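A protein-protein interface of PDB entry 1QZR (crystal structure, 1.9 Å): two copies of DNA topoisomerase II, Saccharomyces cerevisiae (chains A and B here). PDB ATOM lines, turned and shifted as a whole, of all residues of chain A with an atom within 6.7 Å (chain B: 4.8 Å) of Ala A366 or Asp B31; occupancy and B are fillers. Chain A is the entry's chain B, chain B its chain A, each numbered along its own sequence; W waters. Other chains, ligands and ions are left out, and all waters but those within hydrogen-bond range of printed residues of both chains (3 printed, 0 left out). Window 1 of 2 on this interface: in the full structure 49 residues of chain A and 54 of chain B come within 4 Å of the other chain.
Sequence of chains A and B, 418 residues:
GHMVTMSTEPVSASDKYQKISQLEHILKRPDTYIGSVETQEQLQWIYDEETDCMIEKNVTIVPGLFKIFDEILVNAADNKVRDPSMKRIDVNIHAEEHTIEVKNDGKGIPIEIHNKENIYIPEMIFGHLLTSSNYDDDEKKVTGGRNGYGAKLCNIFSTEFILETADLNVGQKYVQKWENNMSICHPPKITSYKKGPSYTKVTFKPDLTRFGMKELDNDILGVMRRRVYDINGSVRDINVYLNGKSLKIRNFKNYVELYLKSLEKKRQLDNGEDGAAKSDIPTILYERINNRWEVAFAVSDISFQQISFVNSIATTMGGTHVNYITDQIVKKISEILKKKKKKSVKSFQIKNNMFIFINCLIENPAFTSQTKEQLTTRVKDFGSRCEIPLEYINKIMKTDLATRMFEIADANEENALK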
ATOM      1  N   ARG A 146      -8.356  -3.400   3.368  1.00  0.00           N
ATOM      2  CA  ARG A 146      -9.530  -2.552   3.458  1.00  0.00           C
ATOM      3  C   ARG A 146      -9.579  -1.737   4.749  1.00  0.00           C
ATOM      4  O   ARG A 146      -9.908  -0.554   4.712  1.00  0.00           O
ATOM      5  CB  ARG A 146     -10.826  -3.376   3.287  1.00  0.00           C
ATOM      6  CG  ARG A 146     -10.990  -4.104   1.927  1.00  0.00           C
ATOM      7  CD  ARG A 146     -11.297  -3.194   0.725  1.00  0.00           C
ATOM      8  NE  ARG A 146     -12.536  -2.455   0.929  1.00  0.00           N
ATOM      9  CZ  ARG A 146     -12.677  -1.148   0.763  1.00  0.00           C
ATOM     10  NH1 ARG A 146     -11.650  -0.401   0.346  1.00  0.00           N
ATOM     11  NH2 ARG A 146     -13.855  -0.584   1.007  1.00  0.00           N
ATOM     12  N   THR A 320     -21.020 -13.576  -2.047  1.00  0.00           N
ATOM     13  CA  THR A 320     -21.817 -13.133  -3.208  1.00  0.00           C
ATOM     14  C   THR A 320     -21.237 -13.494  -4.569  1.00  0.00           C
ATOM     15  O   THR A 320     -21.985 -13.667  -5.533  1.00  0.00           O
ATOM     16  CB  THR A 320     -22.067 -11.627  -3.164  1.00  0.00           C
ATOM     17  OG1 THR A 320     -20.858 -10.961  -2.772  1.00  0.00           O
ATOM     18  CG2 THR A 320     -23.068 -11.284  -2.077  1.00  0.00           C
ATOM     19  N   ILE A 362     -12.508  -7.725  -7.391  1.00  0.00           N
ATOM     20  CA  ILE A 362     -13.714  -6.991  -6.985  1.00  0.00           C
ATOM     21  C   ILE A 362     -13.285  -5.611  -6.469  1.00  0.00           C
ATOM     22  O   ILE A 362     -12.336  -5.499  -5.677  1.00  0.00           O
ATOM     23  CB  ILE A 362     -14.474  -7.750  -5.836  1.00  0.00           C
ATOM     24  CG1 ILE A 362     -14.830  -9.216  -6.219  1.00  0.00           C
ATOM     25  CG2 ILE A 362     -15.702  -6.946  -5.340  1.00  0.00           C
ATOM     26  CD1 ILE A 362     -15.690  -9.369  -7.473  1.00  0.00           C
ATOM     27  N   GLU A 363     -13.988  -4.564  -6.892  1.00  0.00           N
ATOM     28  CA  GLU A 363     -13.669  -3.226  -6.416  1.00  0.00           C
ATOM     29  C   GLU A 363     -14.120  -3.013  -4.983  1.00  0.00           C
ATOM     30  O   GLU A 363     -15.225  -3.406  -4.609  1.00  0.00           O
ATOM     31  CB  GLU A 363     -14.251  -2.155  -7.346  1.00  0.00           C
ATOM     32  CG  GLU A 363     -13.525  -2.098  -8.689  1.00  0.00           C
ATOM     33  CD  GLU A 363     -14.274  -1.312  -9.759  1.00  0.00           C
ATOM     34  OE1 GLU A 363     -15.250  -0.587  -9.431  1.00  0.00           O
ATOM     35  OE2 GLU A 363     -13.886  -1.425 -10.937  1.00  0.00           O
ATOM     36  N   ASN A 364     -13.245  -2.406  -4.182  1.00  0.00           N
ATOM     37  CA  ASN A 364     -13.564  -2.004  -2.809  1.00  0.00           C
ATOM     38  C   ASN A 364     -14.512  -2.978  -2.102  1.00  0.00           C
ATOM     39  O   ASN A 364     -15.605  -2.596  -1.686  1.00  0.00           O
ATOM     40  CB  ASN A 364     -14.127  -0.577  -2.786  1.00  0.00           C
ATOM     41  CG  ASN A 364     -13.134   0.447  -3.301  1.00  0.00           C
ATOM     42  OD1 ASN A 364     -11.946   0.145  -3.502  1.00  0.00           O
ATOM     43  ND2 ASN A 364     -13.613   1.670  -3.532  1.00  0.00           N
ATOM     44  N   PRO A 365     -14.086  -4.232  -1.983  1.00  0.00           N
ATOM     45  CA  PRO A 365     -14.958  -5.308  -1.488  1.00  0.00           C
ATOM     46  C   PRO A 365     -15.357  -5.142  -0.018  1.00  0.00           C
ATOM     47  O   PRO A 365     -14.616  -4.546   0.772  1.00  0.00           O
ATOM     48  CB  PRO A 365     -14.104  -6.561  -1.676  1.00  0.00           C
ATOM     49  CG  PRO A 365     -12.695  -6.077  -1.653  1.00  0.00           C
ATOM     50  CD  PRO A 365     -12.727  -4.725  -2.304  1.00  0.00           C
ATOM     51  N   ALA A 366     -16.521  -5.685   0.338  1.00  0.00           N
ATOM     52  CA  ALA A 366     -16.967  -5.707   1.730  1.00  0.00           C
ATOM     53  C   ALA A 366     -17.097  -7.161   2.165  1.00  0.00           C
ATOM     54  O   ALA A 366     -17.487  -8.026   1.358  1.00  0.00           O
ATOM     55  CB  ALA A 366     -18.298  -4.989   1.871  1.00  0.00           C
ATOM     56  N   PHE A 367     -16.774  -7.426   3.425  1.00  0.00           N
ATOM     57  CA  PHE A 367     -16.830  -8.776   3.988  1.00  0.00           C
ATOM     58  C   PHE A 367     -17.605  -8.777   5.309  1.00  0.00           C
ATOM     59  O   PHE A 367     -17.777  -7.729   5.919  1.00  0.00           O
ATOM     60  CB  PHE A 367     -15.402  -9.327   4.193  1.00  0.00           C
ATOM     61  CG  PHE A 367     -14.580  -9.395   2.913  1.00  0.00           C
ATOM     62  CD1 PHE A 367     -14.547 -10.570   2.147  1.00  0.00           C
ATOM     63  CD2 PHE A 367     -13.840  -8.286   2.476  1.00  0.00           C
ATOM     64  CE1 PHE A 367     -13.794 -10.639   0.967  1.00  0.00           C
ATOM     65  CE2 PHE A 367     -13.076  -8.350   1.295  1.00  0.00           C
ATOM     66  CZ  PHE A 367     -13.062  -9.533   0.541  1.00  0.00           C
ATOM     67  N   THR A 368     -18.052  -9.951   5.761  1.00  0.00           N
ATOM     68  CA  THR A 368     -18.738 -10.046   7.063  1.00  0.00           C
ATOM     69  C   THR A 368     -17.823  -9.706   8.246  1.00  0.00           C
ATOM     70  O   THR A 368     -18.300  -9.269   9.310  1.00  0.00           O
ATOM     71  CB  THR A 368     -19.349 -11.454   7.286  1.00  0.00           C
ATOM     72  OG1 THR A 368     -18.334 -12.447   7.128  1.00  0.00           O
ATOM     73  CG2 THR A 368     -20.348 -11.791   6.214  1.00  0.00           C
ATOM     74  N   SER A 369     -16.518  -9.924   8.090  1.00  0.00           N
ATOM     75  CA  SER A 369     -15.608  -9.700   9.210  1.00  0.00           C
ATOM     76  C   SER A 369     -14.202  -9.339   8.736  1.00  0.00           C
ATOM     77  O   SER A 369     -13.891  -9.424   7.539  1.00  0.00           O
ATOM     78  CB  SER A 369     -15.547 -10.947  10.095  1.00  0.00           C
ATOM     79  OG  SER A 369     -14.785 -11.953   9.454  1.00  0.00           O
ATOM     80  N   GLN A 374     -15.920 -14.266   3.950  1.00  0.00           N
ATOM     81  CA  GLN A 374     -17.204 -14.212   3.219  1.00  0.00           C
ATOM     82  C   GLN A 374     -17.477 -12.834   2.606  1.00  0.00           C
ATOM     83  O   GLN A 374     -17.675 -11.862   3.334  1.00  0.00           O
ATOM     84  CB  GLN A 374     -18.375 -14.611   4.139  1.00  0.00           C
ATOM     85  CG  GLN A 374     -19.697 -14.809   3.401  1.00  0.00           C
ATOM     86  CD  GLN A 374     -20.868 -15.142   4.322  1.00  0.00           C
ATOM     87  OE1 GLN A 374     -20.690 -15.751   5.374  1.00  0.00           O
ATOM     88  NE2 GLN A 374     -22.070 -14.742   3.914  1.00  0.00           N
ATOM     89  N   LEU A 375     -17.500 -12.766   1.270  1.00  0.00           N
ATOM     90  CA  LEU A 375     -17.786 -11.519   0.548  1.00  0.00           C
ATOM     91  C   LEU A 375     -19.282 -11.139   0.629  1.00  0.00           C
ATOM     92  O   LEU A 375     -20.152 -11.992   0.442  1.00  0.00           O
ATOM     93  CB  LEU A 375     -17.362 -11.651  -0.930  1.00  0.00           C
ATOM     94  CG  LEU A 375     -17.490 -10.383  -1.793  1.00  0.00           C
ATOM     95  CD1 LEU A 375     -16.382  -9.385  -1.451  1.00  0.00           C
ATOM     96  CD2 LEU A 375     -17.439 -10.738  -3.288  1.00  0.00           C
ATOM     97  N   THR A 376     -19.564  -9.860   0.889  1.00  0.00           N
ATOM     98  CA  THR A 376     -20.948  -9.372   0.993  1.00  0.00           C
ATOM     99  C   THR A 376     -21.310  -8.335  -0.079  1.00  0.00           C
ATOM    100  O   THR A 376     -22.488  -8.022  -0.267  1.00  0.00           O
ATOM    101  CB  THR A 376     -21.223  -8.761   2.378  1.00  0.00           C
ATOM    102  OG1 THR A 376     -20.234  -7.763   2.661  1.00  0.00           O
ATOM    103  CG2 THR A 376     -21.025  -9.794   3.474  1.00  0.00           C
ATOM    104  N   THR A 377     -20.301  -7.806  -0.774  1.00  0.00           N
ATOM    105  CA  THR A 377     -20.516  -6.848  -1.875  1.00  0.00           C
ATOM    106  C   THR A 377     -21.602  -7.344  -2.842  1.00  0.00           C
ATOM    107  O   THR A 377     -21.572  -8.483  -3.261  1.00  0.00           O
ATOM    108  CB  THR A 377     -19.182  -6.625  -2.638  1.00  0.00           C
ATOM    109  OG1 THR A 377     -18.213  -6.039  -1.749  1.00  0.00           O
ATOM    110  CG2 THR A 377     -19.343  -5.576  -3.753  1.00  0.00           C
ATOM    111  N   ARG B  29     -16.943   2.710   7.718  1.00  0.00           N
ATOM    112  CA  ARG B  29     -16.958   1.304   7.319  1.00  0.00           C
ATOM    113  C   ARG B  29     -17.837   0.486   8.258  1.00  0.00           C
ATOM    114  O   ARG B  29     -17.335  -0.247   9.106  1.00  0.00           O
ATOM    115  CB  ARG B  29     -15.528   0.741   7.311  1.00  0.00           C
ATOM    116  CG  ARG B  29     -14.576   1.465   6.354  1.00  0.00           C
ATOM    117  CD  ARG B  29     -14.902   1.211   4.877  1.00  0.00           C
ATOM    118  NE  ARG B  29     -14.013   1.933   3.979  1.00  0.00           N
ATOM    119  CZ  ARG B  29     -12.740   1.618   3.771  1.00  0.00           C
ATOM    120  NH1 ARG B  29     -12.195   0.585   4.399  1.00  0.00           N
ATOM    121  NH2 ARG B  29     -12.016   2.329   2.928  1.00  0.00           N
ATOM    122  N   PRO B  30     -19.153   0.642   8.127  1.00  0.00           N
ATOM    123  CA  PRO B  30     -20.106  -0.009   9.029  1.00  0.00           C
ATOM    124  C   PRO B  30     -20.133  -1.545   8.947  1.00  0.00           C
ATOM    125  O   PRO B  30     -20.548  -2.180   9.917  1.00  0.00           O
ATOM    126  CB  PRO B  30     -21.453   0.585   8.596  1.00  0.00           C
ATOM    127  CG  PRO B  30     -21.083   1.870   7.888  1.00  0.00           C
ATOM    128  CD  PRO B  30     -19.827   1.504   7.133  1.00  0.00           C
ATOM    129  N   ASP B  31     -19.670  -2.122   7.839  1.00  0.00           N
ATOM    130  CA  ASP B  31     -19.935  -3.539   7.540  1.00  0.00           C
ATOM    131  C   ASP B  31     -19.588  -4.554   8.627  1.00  0.00           C
ATOM    132  O   ASP B  31     -20.393  -5.428   8.923  1.00  0.00           O
ATOM    133  CB  ASP B  31     -19.312  -3.958   6.211  1.00  0.00           C
ATOM    134  CG  ASP B  31     -20.041  -3.380   5.039  1.00  0.00           C
ATOM    135  OD1 ASP B  31     -20.762  -4.127   4.335  1.00  0.00           O
ATOM    136  OD2 ASP B  31     -19.963  -2.165   4.751  1.00  0.00           O
ATOM    137  N   THR B  32     -18.399  -4.458   9.216  1.00  0.00           N
ATOM    138  CA  THR B  32     -18.018  -5.444  10.238  1.00  0.00           C
ATOM    139  C   THR B  32     -18.604  -5.120  11.610  1.00  0.00           C
ATOM    140  O   THR B  32     -18.480  -5.921  12.540  1.00  0.00           O
ATOM    141  CB  THR B  32     -16.497  -5.617  10.354  1.00  0.00           C
ATOM    142  OG1 THR B  32     -15.896  -4.372  10.755  1.00  0.00           O
ATOM    143  CG2 THR B  32     -15.876  -5.932   8.970  1.00  0.00           C
ATOM    144  N   TYR B  33     -19.223  -3.948  11.743  1.00  0.00           N
ATOM    145  CA  TYR B  33     -19.869  -3.586  13.008  1.00  0.00           C
ATOM    146  C   TYR B  33     -21.367  -3.943  13.008  1.00  0.00           C
ATOM    147  O   TYR B  33     -21.849  -4.621  13.925  1.00  0.00           O
ATOM    148  CB  TYR B  33     -19.660  -2.106  13.334  1.00  0.00           C
ATOM    149  CG  TYR B  33     -18.213  -1.663  13.387  1.00  0.00           C
ATOM    150  CD1 TYR B  33     -17.472  -1.755  14.572  1.00  0.00           C
ATOM    151  CD2 TYR B  33     -17.591  -1.125  12.268  1.00  0.00           C
ATOM    152  CE1 TYR B  33     -16.149  -1.323  14.625  1.00  0.00           C
ATOM    153  CE2 TYR B  33     -16.257  -0.701  12.312  1.00  0.00           C
ATOM    154  CZ  TYR B  33     -15.547  -0.810  13.490  1.00  0.00           C
ATOM    155  OH  TYR B  33     -14.236  -0.374  13.538  1.00  0.00           O
ATOM    156  N   ILE B  34     -22.093  -3.499  11.981  1.00  0.00           N
ATOM    157  CA  ILE B  34     -23.564  -3.656  11.936  1.00  0.00           C
ATOM    158  C   ILE B  34     -24.085  -4.308  10.636  1.00  0.00           C
ATOM    159  O   ILE B  34     -25.303  -4.528  10.471  1.00  0.00           O
ATOM    160  CB  ILE B  34     -24.264  -2.281  12.152  1.00  0.00           C
ATOM    161  CG1 ILE B  34     -23.926  -1.297  11.015  1.00  0.00           C
ATOM    162  CG2 ILE B  34     -23.912  -1.695  13.519  1.00  0.00           C
ATOM    163  CD1 ILE B  34     -24.816  -0.047  10.993  1.00  0.00           C
ATOM    164  N   GLY B  35     -23.177  -4.635   9.727  1.00  0.00           N
ATOM    165  CA  GLY B  35     -23.570  -5.177   8.434  1.00  0.00           C
ATOM    166  C   GLY B  35     -23.722  -4.052   7.419  1.00  0.00           C
ATOM    167  O   GLY B  35     -23.426  -2.887   7.714  1.00  0.00           O
ATOM    168  N   SER B  36     -24.180  -4.390   6.223  1.00  0.00           N
ATOM    169  CA  SER B  36     -24.205  -3.430   5.125  1.00  0.00           C
ATOM    170  C   SER B  36     -25.179  -2.263   5.360  1.00  0.00           C
ATOM    171  O   SER B  36     -26.264  -2.452   5.892  1.00  0.00           O
ATOM    172  CB  SER B  36     -24.560  -4.131   3.816  1.00  0.00           C
ATOM    173  OG  SER B  36     -24.562  -3.185   2.761  1.00  0.00           O
HETATM  174  O   HOH W   1     -21.252  -6.791   5.099  1.00  0.00           O
HETATM  175  O   HOH W   2     -20.600  -7.983   9.419  1.00  0.00           O
HETATM  176  O   HOH W   3     -23.349  -4.930   0.159  1.00  0.00           O
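Printed residues of chain B within 4 Å of Arg A146: Arg B29 (2.6 Å).
Asn A364 touches none of the printed residues of chain B.
Ala A366 touches just one residue of chain B: Asp B31.
Of the printed residues of chain B, Ser A369 touches Thr B32.
Asp B31 touches one residue of chain A.
Of the printed residues of chain A, Thr B32 touches Thr A368 (3.9 Å) and Ser A369 (3.8 Å).
Ile B34 touches none of the printed residues of chain A.
The nearest printed residue of chain B that does not touch Ala A366 is Ser B36 (6.6 Å).
O of Pro A365 is in hydrogen-bond range of NE of Arg A146, 3.0 Å away.
The backbone NH of Thr A376 is in hydrogen-bond range of the backbone carbonyl oxygen of Ala A366.
The backbone NH (N) of Ala A366 sits at hydrogen-bond distance from the side-chain hydroxyl (OG1) of Thr A377 (2.7 Å).
The backbone carbonyl oxygen (O) of Gln A374 lies within hydrogen-bond range of the backbone NH (N) of Thr A368, at 3.1 Å.
The guanidinium group of Arg B29 lies within hydrogen-bond range of the backbone carbonyl oxygen of Arg A146 (2.6 Å).
Among the printed residues, merely in contact across the chains: Ala A366 with Asp B31, Ser A369 with Thr B32 and Thr A368 with Thr B32.
Water W2 bridges the backbone carbonyl oxygen of Asp B31 (2.6 Å) and the backbone carbonyl oxygen of Thr A368 (2.6 Å).
Water W1 lies within hydrogen-bond range of OD1 of Asp B31 (2.8 Å) and OG1 of Thr A376 (2.8 Å).
Water W3 lies within hydrogen-bond range of O of Thr A376 and OG of Ser B36.
No position is printed for both chains.
Of the 4 pairs that touch across the chains among the printed residues, none has its exchanged pair printed and touching as well.
Printed residues of chain A that touch a printed residue of chain B: Arg A146, Ala A366, Thr A368 and Ser A369.
Among the printed residues, 4 pairs touch across the chains.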
